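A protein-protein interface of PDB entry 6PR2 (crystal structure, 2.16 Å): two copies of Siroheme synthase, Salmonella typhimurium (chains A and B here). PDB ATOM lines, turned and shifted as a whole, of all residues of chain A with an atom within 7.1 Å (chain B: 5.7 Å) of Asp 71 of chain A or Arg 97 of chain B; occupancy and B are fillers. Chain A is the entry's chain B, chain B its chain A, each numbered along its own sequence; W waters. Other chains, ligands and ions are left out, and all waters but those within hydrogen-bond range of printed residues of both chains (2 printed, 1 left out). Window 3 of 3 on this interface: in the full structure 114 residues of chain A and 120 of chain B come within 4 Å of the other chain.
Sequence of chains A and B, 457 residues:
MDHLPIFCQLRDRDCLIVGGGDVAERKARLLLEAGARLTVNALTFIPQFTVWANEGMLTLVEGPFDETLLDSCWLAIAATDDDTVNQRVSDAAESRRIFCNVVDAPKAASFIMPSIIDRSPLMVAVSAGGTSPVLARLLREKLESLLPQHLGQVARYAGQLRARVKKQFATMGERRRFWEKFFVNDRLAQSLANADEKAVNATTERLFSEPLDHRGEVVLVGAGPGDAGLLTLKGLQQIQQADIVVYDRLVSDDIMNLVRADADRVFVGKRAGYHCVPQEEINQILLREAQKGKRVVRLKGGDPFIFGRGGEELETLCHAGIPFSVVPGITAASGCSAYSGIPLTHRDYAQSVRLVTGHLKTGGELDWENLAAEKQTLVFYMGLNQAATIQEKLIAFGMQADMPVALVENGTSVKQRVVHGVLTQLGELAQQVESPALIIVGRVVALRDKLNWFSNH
N of Ile 98 of chain B is in hydrogen-bond range of O of Ala 93 of chain B, 2.9 Å away.
The backbone carbonyl oxygen (O) of Asp 14 of chain A is in hydrogen-bond range of the backbone NH (N) of Trp 74 of chain A, 2.8 Å away.
Asp 71 of chain A touches one residue of chain B.
Of the printed residues of chain B, Trp 74 of chain A touches Glu 94, Arg 97, Ile 98 and Phe 99.
Printed residues of chain A within 4 Å of Arg 97 of chain B: Asp 71 (3.5 Å), Ser 72 (3.4 Å) and Trp 74 (3.5 Å).
Of the printed residues of chain A, Ile 98 of chain B touches Trp 74.
The nearest printed residue of chain B that does not touch Asp 71 of chain A is Arg 96 of chain B (7.5 Å).
The nearest printed residue of chain B that does not touch Arg 13 of chain A is Phe 99 of chain B (4.3 Å).
Positions printed for both chains: 96, 97 and 98.
Of the 7 pairs that touch across the chains among the printed residues, none has its exchanged pair printed and touching as well.
Asp 71 of chain A touches Arg 97 of chain B.
Arg 97 of chain B touches Ser 72 of chain A (CD to O, 3.4 Å).
CZ2 of Trp 74 of chain A touches OE2 of Glu 94 of chain B (3.6 Å).
Trp 74 of chain A touches Arg 97 of chain B (CH2 to CA, 3.5 Å).
CZ3 of Trp 74 of chain A touches C of Ile 98 of chain B, at 3.7 Å.
Phe 99 of chain B touches Trp 74 of chain A.
NH2 of Arg 13 of chain A is in salt-bridge range of OE1 of Glu 94 of chain B.
Printed residues of chain B that touch a printed residue of chain A: Glu 94, Arg 97, Ile 98 and Phe 99.
Hydrophobic or aromatic side chains of chain B within 4 Å of the printed part of chain A: Phe 99.
Of the 15 printed residues of chain A, 4 touch a printed residue of chain B.
Hydrophobic or aromatic side chains of chain A that line the printed part of chain B: Trp 74.
Among the printed residues, 7 pairs touch across the chains.
Among the printed residues, Asp or Glu carboxylates within 4 Å of a Lys or Arg side-chain nitrogen of the other chain: Arg 13 of chain A with Glu 94 of chain B (2.8 Å).
Water W1 lies within hydrogen-bond range of NE of Arg 97 of chain B (2.5 Å) and O of Cys 73 of chain A (2.8 Å).
Water W2 bridges the backbone carbonyl oxygen (O) of Arg 97 of chain B (2.8 Å) and the backbone carbonyl oxygen (O) of Cys 73 of chain A (3.2 Å).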
ATOM      1  N   ARG A  13      -9.848   5.357   8.068  1.00  0.00           N
ATOM      2  CA  ARG A  13      -8.834   6.223   7.471  1.00  0.00           C
ATOM      3  C   ARG A  13      -7.629   5.383   7.072  1.00  0.00           C
ATOM      4  O   ARG A  13      -7.135   4.579   7.874  1.00  0.00           O
ATOM      5  CB  ARG A  13      -8.419   7.355   8.426  1.00  0.00           C
ATOM      6  CG  ARG A  13      -9.527   8.374   8.557  1.00  0.00           C
ATOM      7  CD  ARG A  13      -9.172   9.643   9.313  1.00  0.00           C
ATOM      8  NE  ARG A  13     -10.149  10.667   8.931  1.00  0.00           N
ATOM      9  CZ  ARG A  13     -11.289  10.905   9.573  1.00  0.00           C
ATOM     10  NH1 ARG A  13     -11.596  10.227  10.666  1.00  0.00           N
ATOM     11  NH2 ARG A  13     -12.125  11.833   9.120  1.00  0.00           N
ATOM     12  N   ASP A  14      -7.173   5.560   5.826  1.00  0.00           N
ATOM     13  CA  ASP A  14      -5.972   4.872   5.338  1.00  0.00           C
ATOM     14  C   ASP A  14      -4.769   5.206   6.210  1.00  0.00           C
ATOM     15  O   ASP A  14      -4.428   6.380   6.388  1.00  0.00           O
ATOM     16  CB  ASP A  14      -5.675   5.275   3.891  1.00  0.00           C
ATOM     17  CG  ASP A  14      -6.707   4.763   2.906  1.00  0.00           C
ATOM     18  OD1 ASP A  14      -7.605   4.010   3.316  1.00  0.00           O
ATOM     19  OD2 ASP A  14      -6.606   5.105   1.708  1.00  0.00           O
ATOM     20  N   LEU A  16      -0.604   3.560   6.864  1.00  0.00           N
ATOM     21  CA  LEU A  16       0.433   2.733   6.268  1.00  0.00           C
ATOM     22  C   LEU A  16       1.474   2.361   7.312  1.00  0.00           C
ATOM     23  O   LEU A  16       2.029   3.232   7.984  1.00  0.00           O
ATOM     24  CB  LEU A  16       1.110   3.454   5.106  1.00  0.00           C
ATOM     25  CG  LEU A  16       2.230   2.675   4.406  1.00  0.00           C
ATOM     26  CD1 LEU A  16       1.701   1.409   3.698  1.00  0.00           C
ATOM     27  CD2 LEU A  16       2.917   3.566   3.395  1.00  0.00           C
ATOM     28  N   ASP A  66       7.039   1.501  -1.429  1.00  0.00           N
ATOM     29  CA  ASP A  66       6.477   2.247  -2.554  1.00  0.00           C
ATOM     30  C   ASP A  66       5.847   3.532  -2.022  1.00  0.00           C
ATOM     31  O   ASP A  66       4.824   3.492  -1.332  1.00  0.00           O
ATOM     32  CB  ASP A  66       5.446   1.407  -3.308  1.00  0.00           C
ATOM     33  CG  ASP A  66       4.663   2.219  -4.337  1.00  0.00           C
ATOM     34  OD1 ASP A  66       5.183   3.243  -4.839  1.00  0.00           O
ATOM     35  OD2 ASP A  66       3.510   1.837  -4.632  1.00  0.00           O
ATOM     36  N   GLU A  67       6.439   4.672  -2.379  1.00  0.00           N
ATOM     37  CA  GLU A  67       5.972   5.957  -1.867  1.00  0.00           C
ATOM     38  C   GLU A  67       4.533   6.272  -2.286  1.00  0.00           C
ATOM     39  O   GLU A  67       3.832   7.026  -1.589  1.00  0.00           O
ATOM     40  CB  GLU A  67       6.922   7.058  -2.326  1.00  0.00           C
ATOM     41  CG  GLU A  67       6.263   8.346  -2.718  1.00  0.00           C
ATOM     42  CD  GLU A  67       7.235   9.359  -3.256  1.00  0.00           C
ATOM     43  OE1 GLU A  67       7.462   9.353  -4.483  1.00  0.00           O
ATOM     44  OE2 GLU A  67       7.799  10.133  -2.454  1.00  0.00           O
ATOM     45  N   THR A  68       4.065   5.701  -3.395  1.00  0.00           N
ATOM     46  CA  THR A  68       2.703   5.974  -3.849  1.00  0.00           C
ATOM     47  C   THR A  68       1.665   5.335  -2.941  1.00  0.00           C
ATOM     48  O   THR A  68       0.493   5.730  -2.985  1.00  0.00           O
ATOM     49  CB  THR A  68       2.491   5.489  -5.286  1.00  0.00           C
ATOM     50  OG1 THR A  68       2.410   4.059  -5.306  1.00  0.00           O
ATOM     51  CG2 THR A  68       3.630   5.933  -6.193  1.00  0.00           C
ATOM     52  N   LEU A  69       2.068   4.360  -2.123  1.00  0.00           N
ATOM     53  CA  LEU A  69       1.174   3.851  -1.092  1.00  0.00           C
ATOM     54  C   LEU A  69       0.799   4.924  -0.069  1.00  0.00           C
ATOM     55  O   LEU A  69      -0.209   4.768   0.624  1.00  0.00           O
ATOM     56  CB  LEU A  69       1.808   2.654  -0.377  1.00  0.00           C
ATOM     57  CG  LEU A  69       2.140   1.377  -1.164  1.00  0.00           C
ATOM     58  CD1 LEU A  69       2.705   0.327  -0.235  1.00  0.00           C
ATOM     59  CD2 LEU A  69       0.926   0.821  -1.908  1.00  0.00           C
ATOM     60  N   LEU A  70       1.577   6.010   0.050  1.00  0.00           N
ATOM     61  CA  LEU A  70       1.191   7.087   0.957  1.00  0.00           C
ATOM     62  C   LEU A  70       0.124   8.012   0.377  1.00  0.00           C
ATOM     63  O   LEU A  70      -0.349   8.896   1.101  1.00  0.00           O
ATOM     64  CB  LEU A  70       2.422   7.907   1.359  1.00  0.00           C
ATOM     65  CG  LEU A  70       3.375   7.181   2.315  1.00  0.00           C
ATOM     66  CD1 LEU A  70       4.686   7.942   2.390  1.00  0.00           C
ATOM     67  CD2 LEU A  70       2.723   7.028   3.713  1.00  0.00           C
ATOM     68  N   ASP A  71      -0.311   7.775  -0.869  1.00  0.00           N
ATOM     69  CA  ASP A  71      -1.128   8.732  -1.626  1.00  0.00           C
ATOM     70  C   ASP A  71      -2.356   9.219  -0.867  1.00  0.00           C
ATOM     71  O   ASP A  71      -2.686  10.410  -0.905  1.00  0.00           O
ATOM     72  CB  ASP A  71      -1.567   8.100  -2.948  1.00  0.00           C
ATOM     73  CG  ASP A  71      -0.517   8.229  -4.021  1.00  0.00           C
ATOM     74  OD1 ASP A  71       0.554   8.777  -3.698  1.00  0.00           O
ATOM     75  OD2 ASP A  71      -0.750   7.773  -5.170  1.00  0.00           O
ATOM     76  N   SER A  72      -3.079   8.308  -0.215  1.00  0.00           N
ATOM     77  CA  SER A  72      -4.330   8.660   0.449  1.00  0.00           C
ATOM     78  C   SER A  72      -4.249   8.465   1.955  1.00  0.00           C
ATOM     79  O   SER A  72      -5.261   8.232   2.611  1.00  0.00           O
ATOM     80  CB  SER A  72      -5.478   7.838  -0.135  1.00  0.00           C
ATOM     81  OG  SER A  72      -5.987   8.459  -1.309  1.00  0.00           O
ATOM     82  N   CYS A  73      -3.046   8.482   2.518  1.00  0.00           N
ATOM     83  CA  CYS A  73      -2.859   8.056   3.896  1.00  0.00           C
ATOM     84  C   CYS A  73      -2.888   9.247   4.846  1.00  0.00           C
ATOM     85  O   CYS A  73      -2.490  10.361   4.498  1.00  0.00           O
ATOM     86  CB  CYS A  73      -1.540   7.297   4.070  1.00  0.00           C
ATOM     87  SG  CYS A  73      -1.560   5.598   3.460  1.00  0.00           S
ATOM     88  N   TRP A  74      -3.340   8.975   6.069  1.00  0.00           N
ATOM     89  CA  TRP A  74      -3.426   9.932   7.162  1.00  0.00           C
ATOM     90  C   TRP A  74      -2.315   9.793   8.189  1.00  0.00           C
ATOM     91  O   TRP A  74      -2.005  10.763   8.885  1.00  0.00           O
ATOM     92  CB  TRP A  74      -4.751   9.765   7.881  1.00  0.00           C
ATOM     93  CG  TRP A  74      -5.934  10.125   7.054  1.00  0.00           C
ATOM     94  CD1 TRP A  74      -6.469   9.414   6.010  1.00  0.00           C
ATOM     95  CD2 TRP A  74      -6.761  11.272   7.229  1.00  0.00           C
ATOM     96  NE1 TRP A  74      -7.572  10.061   5.517  1.00  0.00           N
ATOM     97  CE2 TRP A  74      -7.780  11.204   6.253  1.00  0.00           C
ATOM     98  CE3 TRP A  74      -6.734  12.360   8.114  1.00  0.00           C
ATOM     99  CZ2 TRP A  74      -8.777  12.177   6.149  1.00  0.00           C
ATOM    100  CZ3 TRP A  74      -7.717  13.322   8.016  1.00  0.00           C
ATOM    101  CH2 TRP A  74      -8.732  13.227   7.029  1.00  0.00           C
ATOM    102  N   ARG A  96       4.529  14.958   2.106  1.00  0.00           N
ATOM    103  CA  ARG A  96       3.086  14.893   1.939  1.00  0.00           C
ATOM    104  C   ARG A  96       2.323  15.424   3.142  1.00  0.00           C
ATOM    105  O   ARG A  96       1.091  15.325   3.172  1.00  0.00           O
ATOM    106  CB  ARG A  96       2.674  13.451   1.670  1.00  0.00           C
ATOM    107  CG  ARG A  96       3.049  12.967   0.293  1.00  0.00           C
ATOM    108  CD  ARG A  96       2.934  11.435   0.240  1.00  0.00           C
ATOM    109  NE  ARG A  96       3.083  10.950  -1.124  1.00  0.00           N
ATOM    110  CZ  ARG A  96       4.238  10.897  -1.769  1.00  0.00           C
ATOM    111  NH1 ARG A  96       5.361  11.271  -1.156  1.00  0.00           N
ATOM    112  NH2 ARG A  96       4.252  10.461  -3.024  1.00  0.00           N
ATOM    113  N   ARG A  97       3.024  15.944   4.145  1.00  0.00           N
ATOM    114  CA  ARG A  97       2.398  16.441   5.371  1.00  0.00           C
ATOM    115  C   ARG A  97       1.589  15.336   6.048  1.00  0.00           C
ATOM    116  O   ARG A  97       0.515  15.559   6.601  1.00  0.00           O
ATOM    117  CB  ARG A  97       1.557  17.696   5.089  1.00  0.00           C
ATOM    118  CG  ARG A  97       2.423  18.832   4.499  1.00  0.00           C
ATOM    119  CD  ARG A  97       1.625  19.993   3.914  1.00  0.00           C
ATOM    120  NE  ARG A  97       0.622  19.512   2.976  1.00  0.00           N
ATOM    121  CZ  ARG A  97       0.830  19.322   1.684  1.00  0.00           C
ATOM    122  NH1 ARG A  97       2.008  19.605   1.145  1.00  0.00           N
ATOM    123  NH2 ARG A  97      -0.149  18.847   0.933  1.00  0.00           N
ATOM    124  N   ILE A  98       2.129  14.127   6.032  1.00  0.00           N
ATOM    125  CA  ILE A  98       1.538  13.002   6.733  1.00  0.00           C
ATOM    126  C   ILE A  98       2.329  12.762   8.014  1.00  0.00           C
ATOM    127  O   ILE A  98       3.536  12.508   7.970  1.00  0.00           O
ATOM    128  CB  ILE A  98       1.528  11.751   5.845  1.00  0.00           C
ATOM    129  CG1 ILE A  98       0.664  11.995   4.599  1.00  0.00           C
ATOM    130  CG2 ILE A  98       1.093  10.531   6.652  1.00  0.00           C
ATOM    131  CD1 ILE A  98       0.810  10.884   3.553  1.00  0.00           C
ATOM    132  N   ALA B  92     -13.248  20.889   3.975  1.00  0.00           N
ATOM    133  CA  ALA B  92     -12.014  21.241   3.278  1.00  0.00           C
ATOM    134  C   ALA B  92     -10.820  20.484   3.864  1.00  0.00           C
ATOM    135  O   ALA B  92      -9.942  20.023   3.128  1.00  0.00           O
ATOM    136  CB  ALA B  92     -11.799  22.754   3.367  1.00  0.00           C
ATOM    137  N   ALA B  93     -10.765  20.343   5.186  1.00  0.00           N
ATOM    138  CA  ALA B  93      -9.652  19.606   5.783  1.00  0.00           C
ATOM    139  C   ALA B  93      -9.715  18.117   5.424  1.00  0.00           C
ATOM    140  O   ALA B  93      -8.690  17.498   5.108  1.00  0.00           O
ATOM    141  CB  ALA B  93      -9.655  19.796   7.287  1.00  0.00           C
ATOM    142  N   GLU B  94     -10.914  17.543   5.416  1.00  0.00           N
ATOM    143  CA  GLU B  94     -11.056  16.131   5.080  1.00  0.00           C
ATOM    144  C   GLU B  94     -10.531  15.826   3.684  1.00  0.00           C
ATOM    145  O   GLU B  94      -9.777  14.871   3.497  1.00  0.00           O
ATOM    146  CB  GLU B  94     -12.520  15.717   5.184  1.00  0.00           C
ATOM    147  CG  GLU B  94     -12.813  14.334   4.611  1.00  0.00           C
ATOM    148  CD  GLU B  94     -12.489  13.207   5.588  1.00  0.00           C
ATOM    149  OE1 GLU B  94     -12.525  13.440   6.813  1.00  0.00           O
ATOM    150  OE2 GLU B  94     -12.196  12.084   5.127  1.00  0.00           O
ATOM    151  N   SER B  95     -10.937  16.610   2.681  1.00  0.00           N
ATOM    152  CA  SER B  95     -10.490  16.305   1.328  1.00  0.00           C
ATOM    153  C   SER B  95      -8.970  16.323   1.230  1.00  0.00           C
ATOM    154  O   SER B  95      -8.391  15.541   0.469  1.00  0.00           O
ATOM    155  CB  SER B  95     -11.102  17.287   0.340  1.00  0.00           C
ATOM    156  OG  SER B  95     -10.955  18.602   0.835  1.00  0.00           O
ATOM    157  N   ARG B  96      -8.305  17.164   2.022  1.00  0.00           N
ATOM    158  CA  ARG B  96      -6.845  17.245   2.022  1.00  0.00           C
ATOM    159  C   ARG B  96      -6.192  16.264   2.991  1.00  0.00           C
ATOM    160  O   ARG B  96      -4.963  16.296   3.153  1.00  0.00           O
ATOM    161  CB  ARG B  96      -6.395  18.679   2.378  1.00  0.00           C
ATOM    162  CG  ARG B  96      -6.894  19.741   1.384  1.00  0.00           C
ATOM    163  CD  ARG B  96      -6.596  21.154   1.871  1.00  0.00           C
ATOM    164  NE  ARG B  96      -6.844  22.149   0.830  1.00  0.00           N
ATOM    165  CZ  ARG B  96      -8.049  22.499   0.395  1.00  0.00           C
ATOM    166  NH1 ARG B  96      -9.147  21.936   0.900  1.00  0.00           N
ATOM    167  NH2 ARG B  96      -8.157  23.415  -0.555  1.00  0.00           N
ATOM    168  N   ARG B  97      -6.983  15.424   3.664  1.00  0.00           N
ATOM    169  CA  ARG B  97      -6.477  14.512   4.696  1.00  0.00           C
ATOM    170  C   ARG B  97      -5.675  15.272   5.751  1.00  0.00           C
ATOM    171  O   ARG B  97      -4.574  14.889   6.156  1.00  0.00           O
ATOM    172  CB  ARG B  97      -5.671  13.370   4.066  1.00  0.00           C
ATOM    173  CG  ARG B  97      -6.566  12.507   3.123  1.00  0.00           C
ATOM    174  CD  ARG B  97      -5.765  11.607   2.230  1.00  0.00           C
ATOM    175  NE  ARG B  97      -4.648  12.334   1.635  1.00  0.00           N
ATOM    176  CZ  ARG B  97      -4.721  13.025   0.505  1.00  0.00           C
ATOM    177  NH1 ARG B  97      -5.860  13.081  -0.178  1.00  0.00           N
ATOM    178  NH2 ARG B  97      -3.644  13.656   0.060  1.00  0.00           N
ATOM    179  N   ILE B  98      -6.270  16.348   6.241  1.00  0.00           N
ATOM    180  CA  ILE B  98      -5.714  17.108   7.354  1.00  0.00           C
ATOM    181  C   ILE B  98      -6.567  16.807   8.572  1.00  0.00           C
ATOM    182  O   ILE B  98      -7.789  16.997   8.536  1.00  0.00           O
ATOM    183  CB  ILE B  98      -5.703  18.612   7.042  1.00  0.00           C
ATOM    184  CG1 ILE B  98      -4.799  18.876   5.838  1.00  0.00           C
ATOM    185  CG2 ILE B  98      -5.330  19.437   8.285  1.00  0.00           C
ATOM    186  CD1 ILE B  98      -4.984  20.307   5.232  1.00  0.00           C
ATOM    187  N   PHE B  99      -5.934  16.350   9.654  1.00  0.00           N
ATOM    188  CA  PHE B  99      -6.681  16.136  10.876  1.00  0.00           C
ATOM    189  C   PHE B  99      -7.241  17.469  11.353  1.00  0.00           C
ATOM    190  O   PHE B  99      -6.552  18.491  11.335  1.00  0.00           O
ATOM    191  CB  PHE B  99      -5.792  15.510  11.949  1.00  0.00           C
ATOM    192  CG  PHE B  99      -5.606  14.024  11.801  1.00  0.00           C
ATOM    193  CD1 PHE B  99      -6.664  13.144  12.044  1.00  0.00           C
ATOM    194  CD2 PHE B  99      -4.375  13.506  11.442  1.00  0.00           C
ATOM    195  CE1 PHE B  99      -6.502  11.788  11.921  1.00  0.00           C
ATOM    196  CE2 PHE B  99      -4.188  12.142  11.313  1.00  0.00           C
ATOM    197  CZ  PHE B  99      -5.244  11.268  11.559  1.00  0.00           C
HETATM  198  O   HOH W   1      -2.316  12.380   2.514  1.00  0.00           O
HETATM  199  O   HOH W   2      -2.343  13.220   5.869  1.00  0.00           O
